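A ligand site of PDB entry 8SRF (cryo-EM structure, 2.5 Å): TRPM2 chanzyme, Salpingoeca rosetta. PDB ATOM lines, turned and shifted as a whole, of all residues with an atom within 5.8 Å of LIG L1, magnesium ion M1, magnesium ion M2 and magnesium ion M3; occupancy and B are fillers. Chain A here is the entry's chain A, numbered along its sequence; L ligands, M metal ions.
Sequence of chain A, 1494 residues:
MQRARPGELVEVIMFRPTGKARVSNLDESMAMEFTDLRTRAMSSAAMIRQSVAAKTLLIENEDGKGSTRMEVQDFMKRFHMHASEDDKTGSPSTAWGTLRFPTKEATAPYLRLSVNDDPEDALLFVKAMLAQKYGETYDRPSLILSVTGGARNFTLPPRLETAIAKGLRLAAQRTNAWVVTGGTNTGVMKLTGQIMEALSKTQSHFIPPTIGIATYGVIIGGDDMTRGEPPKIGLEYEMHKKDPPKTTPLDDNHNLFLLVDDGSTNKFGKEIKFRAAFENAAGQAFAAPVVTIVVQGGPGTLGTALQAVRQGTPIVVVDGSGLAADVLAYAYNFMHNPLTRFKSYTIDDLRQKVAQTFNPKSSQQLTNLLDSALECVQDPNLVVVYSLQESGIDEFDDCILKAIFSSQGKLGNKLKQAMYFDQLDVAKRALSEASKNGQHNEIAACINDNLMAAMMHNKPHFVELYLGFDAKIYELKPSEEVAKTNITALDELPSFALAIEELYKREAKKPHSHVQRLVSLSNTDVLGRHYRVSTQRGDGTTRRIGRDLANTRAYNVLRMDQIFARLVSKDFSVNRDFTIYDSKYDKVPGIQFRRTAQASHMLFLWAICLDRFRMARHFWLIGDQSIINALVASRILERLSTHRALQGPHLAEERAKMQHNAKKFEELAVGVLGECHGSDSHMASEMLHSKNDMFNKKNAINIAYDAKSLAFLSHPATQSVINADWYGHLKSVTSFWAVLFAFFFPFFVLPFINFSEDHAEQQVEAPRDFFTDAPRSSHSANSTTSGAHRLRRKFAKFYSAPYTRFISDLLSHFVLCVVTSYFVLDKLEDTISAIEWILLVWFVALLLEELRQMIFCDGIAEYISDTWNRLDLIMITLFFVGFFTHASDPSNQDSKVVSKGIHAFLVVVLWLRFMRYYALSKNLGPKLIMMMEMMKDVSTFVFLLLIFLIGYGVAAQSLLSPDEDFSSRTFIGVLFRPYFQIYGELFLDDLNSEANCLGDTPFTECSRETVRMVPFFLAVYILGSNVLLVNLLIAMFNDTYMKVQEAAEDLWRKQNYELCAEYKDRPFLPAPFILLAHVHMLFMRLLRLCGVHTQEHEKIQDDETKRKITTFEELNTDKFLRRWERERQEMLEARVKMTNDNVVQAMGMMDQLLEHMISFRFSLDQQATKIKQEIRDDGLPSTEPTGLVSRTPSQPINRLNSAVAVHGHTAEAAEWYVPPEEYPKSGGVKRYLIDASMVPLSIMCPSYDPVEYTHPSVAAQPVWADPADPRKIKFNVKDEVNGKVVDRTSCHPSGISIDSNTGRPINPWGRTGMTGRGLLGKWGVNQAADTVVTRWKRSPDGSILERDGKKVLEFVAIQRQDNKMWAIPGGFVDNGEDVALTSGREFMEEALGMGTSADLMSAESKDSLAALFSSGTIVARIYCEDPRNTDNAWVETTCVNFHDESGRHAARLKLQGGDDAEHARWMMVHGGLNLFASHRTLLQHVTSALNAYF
Arg 1385 touches magnesium ion M3.
Merely in contact with magnesium ion M2: Asp 1459. Four residues have an atom within 4 Å of magnesium ion M2: Glu 1386, Glu 1390, Asp 1459 and Asp 1460. Along chain A the residues within 4 Å of magnesium ion M2 span positions 1386 to 1460.
Magnesium ion M1 is bound by an oxygen (O5) of LG2 L2, the side-chain carboxylate (OE2) of Glu 1390, an oxygen (O2) of LIG L1 and the side-chain carboxylate (OD2) of Asp 1460. Magnesium ion M1 has four donor atoms within binding distance. Slightly farther from magnesium ion M1 lies O of Gly 1370 (2.8 Å).
O3 of LIG L1 binds magnesium ion M3. OE2 of Glu 1386 is bound to magnesium ion M3 (2.5 Å). Magnesium ion M3 has two donor atoms within binding distance.
The side-chain amide oxygen (OD1) of Asn 1326 sits at hydrogen-bond distance from a nitrogen (N3) of LIG L1 (2.9 Å). A nitrogen (N4) of LIG L1 is in hydrogen-bond range of the backbone NH (N) of Gly 1321, at 3.3 Å. NH2 of Arg 1360 is in salt-bridge range of O6 of LG2 L2 (2.6 Å). O6 of LG2 L2 is in salt-bridge range of NH1 of Arg 1428, at 3.0 Å.
Along chain A the residues within 4 Å of magnesium ion M1 span positions 1370 to 1460.
Trp 1264 touches LIG L1 (CZ2 to O7, 3.4 Å). O of Leu 1319 touches C9 of LIG L1 (3.7 Å). CA of Leu 1320 touches C9 of LIG L1 (3.9 Å). Lys 1322 touches LIG L1. Gly 1371 touches LIG L1. CG of Phe 1372 touches C8 of LIG L1 (3.4 Å). Asp 1459 touches LIG L1. The nearest printed residue that does not touch LIG L1 is Asp 1374 (4.4 Å).
The backbone NH of Gly 1370 lies within hydrogen-bond range of the side-chain carboxylate of Glu 1390. OE2 of Glu 1386 lies close to NH1 of Arg 1385 (2.6 Å). O of Lys 1322 sits at hydrogen-bond distance from ND2 of Asn 1326 (2.7 Å). The guanidinium group of Arg 1385 lies within salt-bridge range of the side-chain carboxylate of Asp 1374 (3.5 Å). NH1 of Arg 1385 lies within salt-bridge range of OE1 of Glu 1389, 3.7 Å away. O of Trp 1264 lies within hydrogen-bond range of NZ of Lys 1322 (3.1 Å).
Magnesium ion M2 is bound by the side-chain carboxylate of Glu 1390 (2.1 Å), an oxygen (O1) of LIG L1 (2.1 Å), the side-chain carboxylate of Glu 1386 (2.1 Å), an oxygen (O2) of LIG L1 (2.2 Å) and the side-chain carboxylate of Asp 1460 (2.4 Å). Magnesium ion M2 has five donor atoms within binding distance.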
ATOM      1  N   LYS A1225     -29.687 -37.557  15.737  1.00  0.00           N
ATOM      2  CA  LYS A1225     -30.873 -36.714  15.395  1.00  0.00           C
ATOM      3  C   LYS A1225     -30.710 -35.867  14.109  1.00  0.00           C
ATOM      4  O   LYS A1225     -31.346 -34.827  13.956  1.00  0.00           O
ATOM      5  CB  LYS A1225     -31.273 -35.826  16.580  1.00  0.00           C
ATOM      6  CG  LYS A1225     -31.680 -36.594  17.821  1.00  0.00           C
ATOM      7  CD  LYS A1225     -32.471 -35.726  18.776  1.00  0.00           C
ATOM      8  CE  LYS A1225     -31.579 -34.724  19.487  1.00  0.00           C
ATOM      9  NZ  LYS A1225     -32.333 -33.889  20.472  1.00  0.00           N
ATOM     10  N   TRP A1264     -30.146 -19.224  22.904  1.00  0.00           N
ATOM     11  CA  TRP A1264     -28.914 -19.819  23.420  1.00  0.00           C
ATOM     12  C   TRP A1264     -27.918 -20.164  22.323  1.00  0.00           C
ATOM     13  O   TRP A1264     -26.908 -20.812  22.606  1.00  0.00           O
ATOM     14  CB  TRP A1264     -29.229 -21.107  24.196  1.00  0.00           C
ATOM     15  CG  TRP A1264     -30.263 -22.015  23.559  1.00  0.00           C
ATOM     16  CD1 TRP A1264     -31.612 -22.012  23.791  1.00  0.00           C
ATOM     17  CD2 TRP A1264     -30.042 -23.019  22.561  1.00  0.00           C
ATOM     18  NE1 TRP A1264     -32.235 -22.959  23.033  1.00  0.00           N
ATOM     19  CE2 TRP A1264     -31.293 -23.595  22.265  1.00  0.00           C
ATOM     20  CE3 TRP A1264     -28.896 -23.499  21.896  1.00  0.00           C
ATOM     21  CZ2 TRP A1264     -31.440 -24.623  21.319  1.00  0.00           C
ATOM     22  CZ3 TRP A1264     -29.035 -24.526  20.968  1.00  0.00           C
ATOM     23  CH2 TRP A1264     -30.310 -25.074  20.691  1.00  0.00           C
ATOM     24  N   LEU A1319     -25.404 -30.024  16.383  1.00  0.00           N
ATOM     25  CA  LEU A1319     -26.474 -29.843  17.357  1.00  0.00           C
ATOM     26  C   LEU A1319     -26.109 -28.876  18.477  1.00  0.00           C
ATOM     27  O   LEU A1319     -26.984 -28.541  19.288  1.00  0.00           O
ATOM     28  CB  LEU A1319     -26.846 -31.173  18.008  1.00  0.00           C
ATOM     29  CG  LEU A1319     -27.896 -32.074  17.387  1.00  0.00           C
ATOM     30  CD1 LEU A1319     -27.800 -33.438  18.023  1.00  0.00           C
ATOM     31  CD2 LEU A1319     -29.255 -31.483  17.669  1.00  0.00           C
ATOM     32  N   LEU A1320     -24.866 -28.429  18.535  1.00  0.00           N
ATOM     33  CA  LEU A1320     -24.401 -27.564  19.609  1.00  0.00           C
ATOM     34  C   LEU A1320     -24.618 -26.114  19.212  1.00  0.00           C
ATOM     35  O   LEU A1320     -24.345 -25.725  18.077  1.00  0.00           O
ATOM     36  CB  LEU A1320     -22.929 -27.843  19.881  1.00  0.00           C
ATOM     37  CG  LEU A1320     -22.668 -29.297  20.294  1.00  0.00           C
ATOM     38  CD1 LEU A1320     -21.216 -29.492  20.559  1.00  0.00           C
ATOM     39  CD2 LEU A1320     -23.483 -29.747  21.499  1.00  0.00           C
ATOM     40  N   GLY A1321     -25.112 -25.310  20.158  1.00  0.00           N
ATOM     41  CA  GLY A1321     -25.521 -23.959  19.822  1.00  0.00           C
ATOM     42  C   GLY A1321     -24.408 -22.939  19.838  1.00  0.00           C
ATOM     43  O   GLY A1321     -24.532 -21.904  19.176  1.00  0.00           O
ATOM     44  N   LYS A1322     -23.320 -23.217  20.536  1.00  0.00           N
ATOM     45  CA  LYS A1322     -22.247 -22.250  20.711  1.00  0.00           C
ATOM     46  C   LYS A1322     -20.987 -22.712  19.989  1.00  0.00           C
ATOM     47  O   LYS A1322     -20.660 -23.906  20.026  1.00  0.00           O
ATOM     48  CB  LYS A1322     -21.953 -22.027  22.190  1.00  0.00           C
ATOM     49  CG  LYS A1322     -23.132 -21.495  22.984  1.00  0.00           C
ATOM     50  CD  LYS A1322     -22.766 -21.262  24.433  1.00  0.00           C
ATOM     51  CE  LYS A1322     -24.010 -21.064  25.282  1.00  0.00           C
ATOM     52  NZ  LYS A1322     -24.870 -19.970  24.752  1.00  0.00           N
ATOM     53  N   ASN A1326     -18.677 -25.553  24.417  1.00  0.00           N
ATOM     54  CA  ASN A1326     -19.973 -25.585  25.060  1.00  0.00           C
ATOM     55  C   ASN A1326     -19.763 -26.061  26.490  1.00  0.00           C
ATOM     56  O   ASN A1326     -19.392 -27.218  26.713  1.00  0.00           O
ATOM     57  CB  ASN A1326     -20.936 -26.479  24.297  1.00  0.00           C
ATOM     58  CG  ASN A1326     -21.483 -25.823  23.048  1.00  0.00           C
ATOM     59  OD1 ASN A1326     -22.598 -25.306  23.040  1.00  0.00           O
ATOM     60  ND2 ASN A1326     -20.683 -25.822  21.991  1.00  0.00           N
ATOM     61  N   ILE A1358     -30.167 -40.465  35.332  1.00  0.00           N
ATOM     62  CA  ILE A1358     -31.331 -40.189  34.503  1.00  0.00           C
ATOM     63  C   ILE A1358     -31.211 -40.905  33.153  1.00  0.00           C
ATOM     64  O   ILE A1358     -30.126 -41.254  32.689  1.00  0.00           O
ATOM     65  CB  ILE A1358     -31.535 -38.668  34.313  1.00  0.00           C
ATOM     66  CG1 ILE A1358     -30.351 -38.036  33.565  1.00  0.00           C
ATOM     67  CG2 ILE A1358     -31.824 -37.997  35.637  1.00  0.00           C
ATOM     68  CD1 ILE A1358     -30.645 -36.850  32.780  1.00  0.00           C
ATOM     69  N   ARG A1360     -31.854 -40.458  29.427  1.00  0.00           N
ATOM     70  CA  ARG A1360     -31.972 -39.345  28.489  1.00  0.00           C
ATOM     71  C   ARG A1360     -33.119 -39.554  27.505  1.00  0.00           C
ATOM     72  O   ARG A1360     -33.441 -40.687  27.132  1.00  0.00           O
ATOM     73  CB  ARG A1360     -30.666 -39.147  27.735  1.00  0.00           C
ATOM     74  CG  ARG A1360     -29.479 -38.882  28.635  1.00  0.00           C
ATOM     75  CD  ARG A1360     -28.230 -38.674  27.817  1.00  0.00           C
ATOM     76  NE  ARG A1360     -28.411 -37.674  26.770  1.00  0.00           N
ATOM     77  CZ  ARG A1360     -28.234 -36.364  26.933  1.00  0.00           C
ATOM     78  NH1 ARG A1360     -27.871 -35.856  28.100  1.00  0.00           N
ATOM     79  NH2 ARG A1360     -28.421 -35.555  25.909  1.00  0.00           N
ATOM     80  N   GLY A1370     -27.408 -33.040  34.095  1.00  0.00           N
ATOM     81  CA  GLY A1370     -26.590 -31.882  33.791  1.00  0.00           C
ATOM     82  C   GLY A1370     -27.050 -31.280  32.488  1.00  0.00           C
ATOM     83  O   GLY A1370     -27.911 -31.813  31.784  1.00  0.00           O
ATOM     84  N   GLY A1371     -26.435 -30.146  32.171  1.00  0.00           N
ATOM     85  CA  GLY A1371     -26.835 -29.460  30.969  1.00  0.00           C
ATOM     86  C   GLY A1371     -25.903 -28.317  30.663  1.00  0.00           C
ATOM     87  O   GLY A1371     -24.939 -28.062  31.405  1.00  0.00           O
ATOM     88  N   PHE A1372     -26.146 -27.707  29.499  1.00  0.00           N
ATOM     89  CA  PHE A1372     -25.321 -26.618  29.002  1.00  0.00           C
ATOM     90  C   PHE A1372     -25.478 -25.360  29.842  1.00  0.00           C
ATOM     91  O   PHE A1372     -26.562 -25.053  30.340  1.00  0.00           O
ATOM     92  CB  PHE A1372     -25.658 -26.348  27.537  1.00  0.00           C
ATOM     93  CG  PHE A1372     -25.312 -27.484  26.646  1.00  0.00           C
ATOM     94  CD1 PHE A1372     -23.966 -27.759  26.343  1.00  0.00           C
ATOM     95  CD2 PHE A1372     -26.319 -28.330  26.157  1.00  0.00           C
ATOM     96  CE1 PHE A1372     -23.621 -28.829  25.513  1.00  0.00           C
ATOM     97  CE2 PHE A1372     -25.996 -29.423  25.326  1.00  0.00           C
ATOM     98  CZ  PHE A1372     -24.649 -29.662  25.011  1.00  0.00           C
ATOM     99  N   VAL A1373     -24.371 -24.647  30.039  1.00  0.00           N
ATOM    100  CA  VAL A1373     -24.367 -23.404  30.805  1.00  0.00           C
ATOM    101  C   VAL A1373     -25.000 -22.278  30.009  1.00  0.00           C
ATOM    102  O   VAL A1373     -24.582 -21.980  28.886  1.00  0.00           O
ATOM    103  CB  VAL A1373     -22.937 -23.056  31.257  1.00  0.00           C
ATOM    104  CG1 VAL A1373     -22.804 -21.617  31.755  1.00  0.00           C
ATOM    105  CG2 VAL A1373     -22.456 -24.033  32.311  1.00  0.00           C
ATOM    106  N   ASP A1374     -26.066 -21.692  30.561  1.00  0.00           N
ATOM    107  CA  ASP A1374     -26.793 -20.593  29.945  1.00  0.00           C
ATOM    108  C   ASP A1374     -25.965 -19.295  30.019  1.00  0.00           C
ATOM    109  O   ASP A1374     -24.980 -19.194  30.760  1.00  0.00           O
ATOM    110  CB  ASP A1374     -28.141 -20.399  30.631  1.00  0.00           C
ATOM    111  CG  ASP A1374     -29.196 -21.360  30.124  1.00  0.00           C
ATOM    112  OD1 ASP A1374     -28.970 -21.984  29.061  1.00  0.00           O
ATOM    113  OD2 ASP A1374     -30.245 -21.499  30.781  1.00  0.00           O
ATOM    114  N   ARG A1385     -29.974 -25.885  38.996  1.00  0.00           N
ATOM    115  CA  ARG A1385     -31.144 -25.730  38.122  1.00  0.00           C
ATOM    116  C   ARG A1385     -31.398 -26.953  37.250  1.00  0.00           C
ATOM    117  O   ARG A1385     -32.551 -27.390  37.134  1.00  0.00           O
ATOM    118  CB  ARG A1385     -30.961 -24.472  37.260  1.00  0.00           C
ATOM    119  CG  ARG A1385     -32.145 -24.143  36.350  1.00  0.00           C
ATOM    120  CD  ARG A1385     -31.843 -22.936  35.475  1.00  0.00           C
ATOM    121  NE  ARG A1385     -30.503 -22.965  34.881  1.00  0.00           N
ATOM    122  CZ  ARG A1385     -30.171 -23.613  33.776  1.00  0.00           C
ATOM    123  NH1 ARG A1385     -31.049 -24.330  33.088  1.00  0.00           N
ATOM    124  NH2 ARG A1385     -28.925 -23.542  33.334  1.00  0.00           N
ATOM    125  N   GLU A1386     -30.332 -27.520  36.644  1.00  0.00           N
ATOM    126  CA  GLU A1386     -30.437 -28.741  35.820  1.00  0.00           C
ATOM    127  C   GLU A1386     -30.797 -29.959  36.644  1.00  0.00           C
ATOM    128  O   GLU A1386     -31.451 -30.873  36.113  1.00  0.00           O
ATOM    129  CB  GLU A1386     -29.208 -28.989  34.948  1.00  0.00           C
ATOM    130  CG  GLU A1386     -28.990 -28.016  33.752  1.00  0.00           C
ATOM    131  CD  GLU A1386     -30.184 -27.858  32.801  1.00  0.00           C
ATOM    132  OE1 GLU A1386     -30.842 -28.858  32.460  1.00  0.00           O
ATOM    133  OE2 GLU A1386     -30.443 -26.709  32.382  1.00  0.00           O
ATOM    134  N   GLU A1389     -34.501 -29.483  37.458  1.00  0.00           N
ATOM    135  CA  GLU A1389     -35.305 -29.689  36.249  1.00  0.00           C
ATOM    136  C   GLU A1389     -35.351 -31.143  35.792  1.00  0.00           C
ATOM    137  O   GLU A1389     -36.402 -31.634  35.377  1.00  0.00           O
ATOM    138  CB  GLU A1389     -34.834 -28.787  35.105  1.00  0.00           C
ATOM    139  CG  GLU A1389     -35.311 -27.341  35.212  1.00  0.00           C
ATOM    140  CD  GLU A1389     -34.581 -26.420  34.255  1.00  0.00           C
ATOM    141  OE1 GLU A1389     -33.721 -26.904  33.489  1.00  0.00           O
ATOM    142  OE2 GLU A1389     -34.878 -25.210  34.258  1.00  0.00           O
ATOM    143  N   GLU A1390     -34.204 -31.836  35.806  1.00  0.00           N
ATOM    144  CA  GLU A1390     -34.121 -33.174  35.226  1.00  0.00           C
ATOM    145  C   GLU A1390     -34.415 -34.284  36.223  1.00  0.00           C
ATOM    146  O   GLU A1390     -35.288 -35.130  35.950  1.00  0.00           O
ATOM    147  CB  GLU A1390     -32.749 -33.344  34.584  1.00  0.00           C
ATOM    148  CG  GLU A1390     -32.569 -32.445  33.363  1.00  0.00           C
ATOM    149  CD  GLU A1390     -31.209 -32.581  32.713  1.00  0.00           C
ATOM    150  OE1 GLU A1390     -30.449 -33.487  33.089  1.00  0.00           O
ATOM    151  OE2 GLU A1390     -30.908 -31.779  31.816  1.00  0.00           O
ATOM    152  N   ARG A1428     -22.071 -35.724  19.714  1.00  0.00           N
ATOM    153  CA  ARG A1428     -22.481 -34.528  18.986  1.00  0.00           C
ATOM    154  C   ARG A1428     -21.338 -33.543  18.733  1.00  0.00           C
ATOM    155  O   ARG A1428     -21.609 -32.476  18.183  1.00  0.00           O
ATOM    156  CB  ARG A1428     -23.573 -33.759  19.734  1.00  0.00           C
ATOM    157  CG  ARG A1428     -24.787 -34.560  20.092  1.00  0.00           C
ATOM    158  CD  ARG A1428     -25.593 -33.832  21.147  1.00  0.00           C
ATOM    159  NE  ARG A1428     -24.915 -33.856  22.440  1.00  0.00           N
ATOM    160  CZ  ARG A1428     -25.407 -33.344  23.552  1.00  0.00           C
ATOM    161  NH1 ARG A1428     -26.585 -32.737  23.565  1.00  0.00           N
ATOM    162  NH2 ARG A1428     -24.703 -33.429  24.676  1.00  0.00           N
ATOM    163  N   ASP A1459     -38.354 -32.624  32.244  1.00  0.00           N
ATOM    164  CA  ASP A1459     -37.718 -31.825  31.157  1.00  0.00           C
ATOM    165  C   ASP A1459     -37.136 -32.791  30.130  1.00  0.00           C
ATOM    166  O   ASP A1459     -37.914 -33.529  29.499  1.00  0.00           O
ATOM    167  CB  ASP A1459     -36.747 -30.814  31.782  1.00  0.00           C
ATOM    168  CG  ASP A1459     -36.321 -29.725  30.809  1.00  0.00           C
ATOM    169  OD1 ASP A1459     -37.021 -29.530  29.797  1.00  0.00           O
ATOM    170  OD2 ASP A1459     -35.286 -29.070  31.048  1.00  0.00           O
ATOM    171  N   ASP A1460     -35.818 -32.830  29.912  1.00  0.00           N
ATOM    172  CA  ASP A1460     -35.217 -33.695  28.904  1.00  0.00           C
ATOM    173  C   ASP A1460     -34.684 -35.002  29.512  1.00  0.00           C
ATOM    174  O   ASP A1460     -33.717 -35.571  29.000  1.00  0.00           O
ATOM    175  CB  ASP A1460     -34.124 -32.919  28.153  1.00  0.00           C
ATOM    176  CG  ASP A1460     -32.992 -32.465  29.065  1.00  0.00           C
ATOM    177  OD1 ASP A1460     -33.238 -31.601  29.930  1.00  0.00           O
ATOM    178  OD2 ASP A1460     -31.858 -32.965  28.914  1.00  0.00           O
HETATM  179  P1  LIG L   1     -30.436 -28.804  28.989  1.00  0.00           P
HETATM  180  O1  LIG L   1     -31.922 -28.745  29.208  1.00  0.00           O
HETATM  181  O2  LIG L   1     -29.915 -30.106  29.547  1.00  0.00           O
HETATM  182  O3  LIG L   1     -29.831 -27.518  29.488  1.00  0.00           O
HETATM  183  O4  LIG L   1     -30.166 -28.881  27.426  1.00  0.00           O
HETATM  184  C1  LIG L   1     -31.079 -29.528  26.565  1.00  0.00           C
HETATM  185  C2  LIG L   1     -31.604 -28.574  25.529  1.00  0.00           C
HETATM  186  O5  LIG L   1     -31.227 -27.219  25.890  1.00  0.00           O
HETATM  187  C3  LIG L   1     -31.056 -28.731  24.118  1.00  0.00           C
HETATM  188  O6  LIG L   1     -31.679 -29.784  23.408  1.00  0.00           O
HETATM  189  C4  LIG L   1     -31.292 -27.359  23.516  1.00  0.00           C
HETATM  190  O7  LIG L   1     -32.643 -27.199  23.136  1.00  0.00           O
HETATM  191  C5  LIG L   1     -31.010 -26.451  24.727  1.00  0.00           C
HETATM  192  N1  LIG L   1     -29.650 -25.870  24.784  1.00  0.00           N
HETATM  193  C6  LIG L   1     -29.393 -24.868  25.622  1.00  0.00           C
HETATM  194  N2  LIG L   1     -28.113 -24.502  25.518  1.00  0.00           N
HETATM  195  C7  LIG L   1     -27.555 -25.295  24.599  1.00  0.00           C
HETATM  196  C8  LIG L   1     -26.271 -25.359  24.106  1.00  0.00           C
HETATM  197  N3  LIG L   1     -25.063 -24.602  24.388  1.00  0.00           N
HETATM  198  N4  LIG L   1     -25.916 -26.241  23.187  1.00  0.00           N
HETATM  199  C9  LIG L   1     -26.818 -27.124  22.690  1.00  0.00           C
HETATM  200  N5  LIG L   1     -28.078 -27.051  23.184  1.00  0.00           N
HETATM  201  C10 LIG L   1     -28.483 -26.157  24.133  1.00  0.00           C
HETATM  202  C1  LG2 L   2     -22.406 -34.472  28.185  1.00  0.00           C
HETATM  203  O1  LG2 L   2     -23.631 -34.026  27.448  1.00  0.00           O
HETATM  204  C2  LG2 L   2     -22.320 -33.418  29.381  1.00  0.00           C
HETATM  205  O2  LG2 L   2     -21.499 -33.986  30.504  1.00  0.00           O
HETATM  206  C3  LG2 L   2     -23.504 -33.283  29.712  1.00  0.00           C
HETATM  207  O3  LG2 L   2     -23.852 -34.252  30.777  1.00  0.00           O
HETATM  208  C4  LG2 L   2     -24.438 -33.606  28.378  1.00  0.00           C
HETATM  209  C5  LG2 L   2     -25.130 -32.350  27.956  1.00  0.00           C
HETATM  210  O4  LG2 L   2     -26.369 -32.308  28.595  1.00  0.00           O
HETATM  211  P1  LG2 L   2     -27.705 -32.447  27.662  1.00  0.00           P
HETATM  212  O5  LG2 L   2     -28.806 -33.109  28.444  1.00  0.00           O
HETATM  213  O6  LG2 L   2     -27.389 -33.276  26.444  1.00  0.00           O
HETATM  214  O7  LG2 L   2     -28.136 -31.072  27.237  1.00  0.00           O
HETATM  215  O8  LG2 L   2     -21.372 -34.379  27.449  1.00  0.00           O
HETATM  216 MG    MG M   1     -29.984 -32.201  29.953  1.00  0.00          MG
HETATM  217 MG    MG M   2     -31.675 -30.033  30.881  1.00  0.00          MG
HETATM  218 MG    MG M   3     -30.909 -25.769  30.082  1.00  0.00          MG
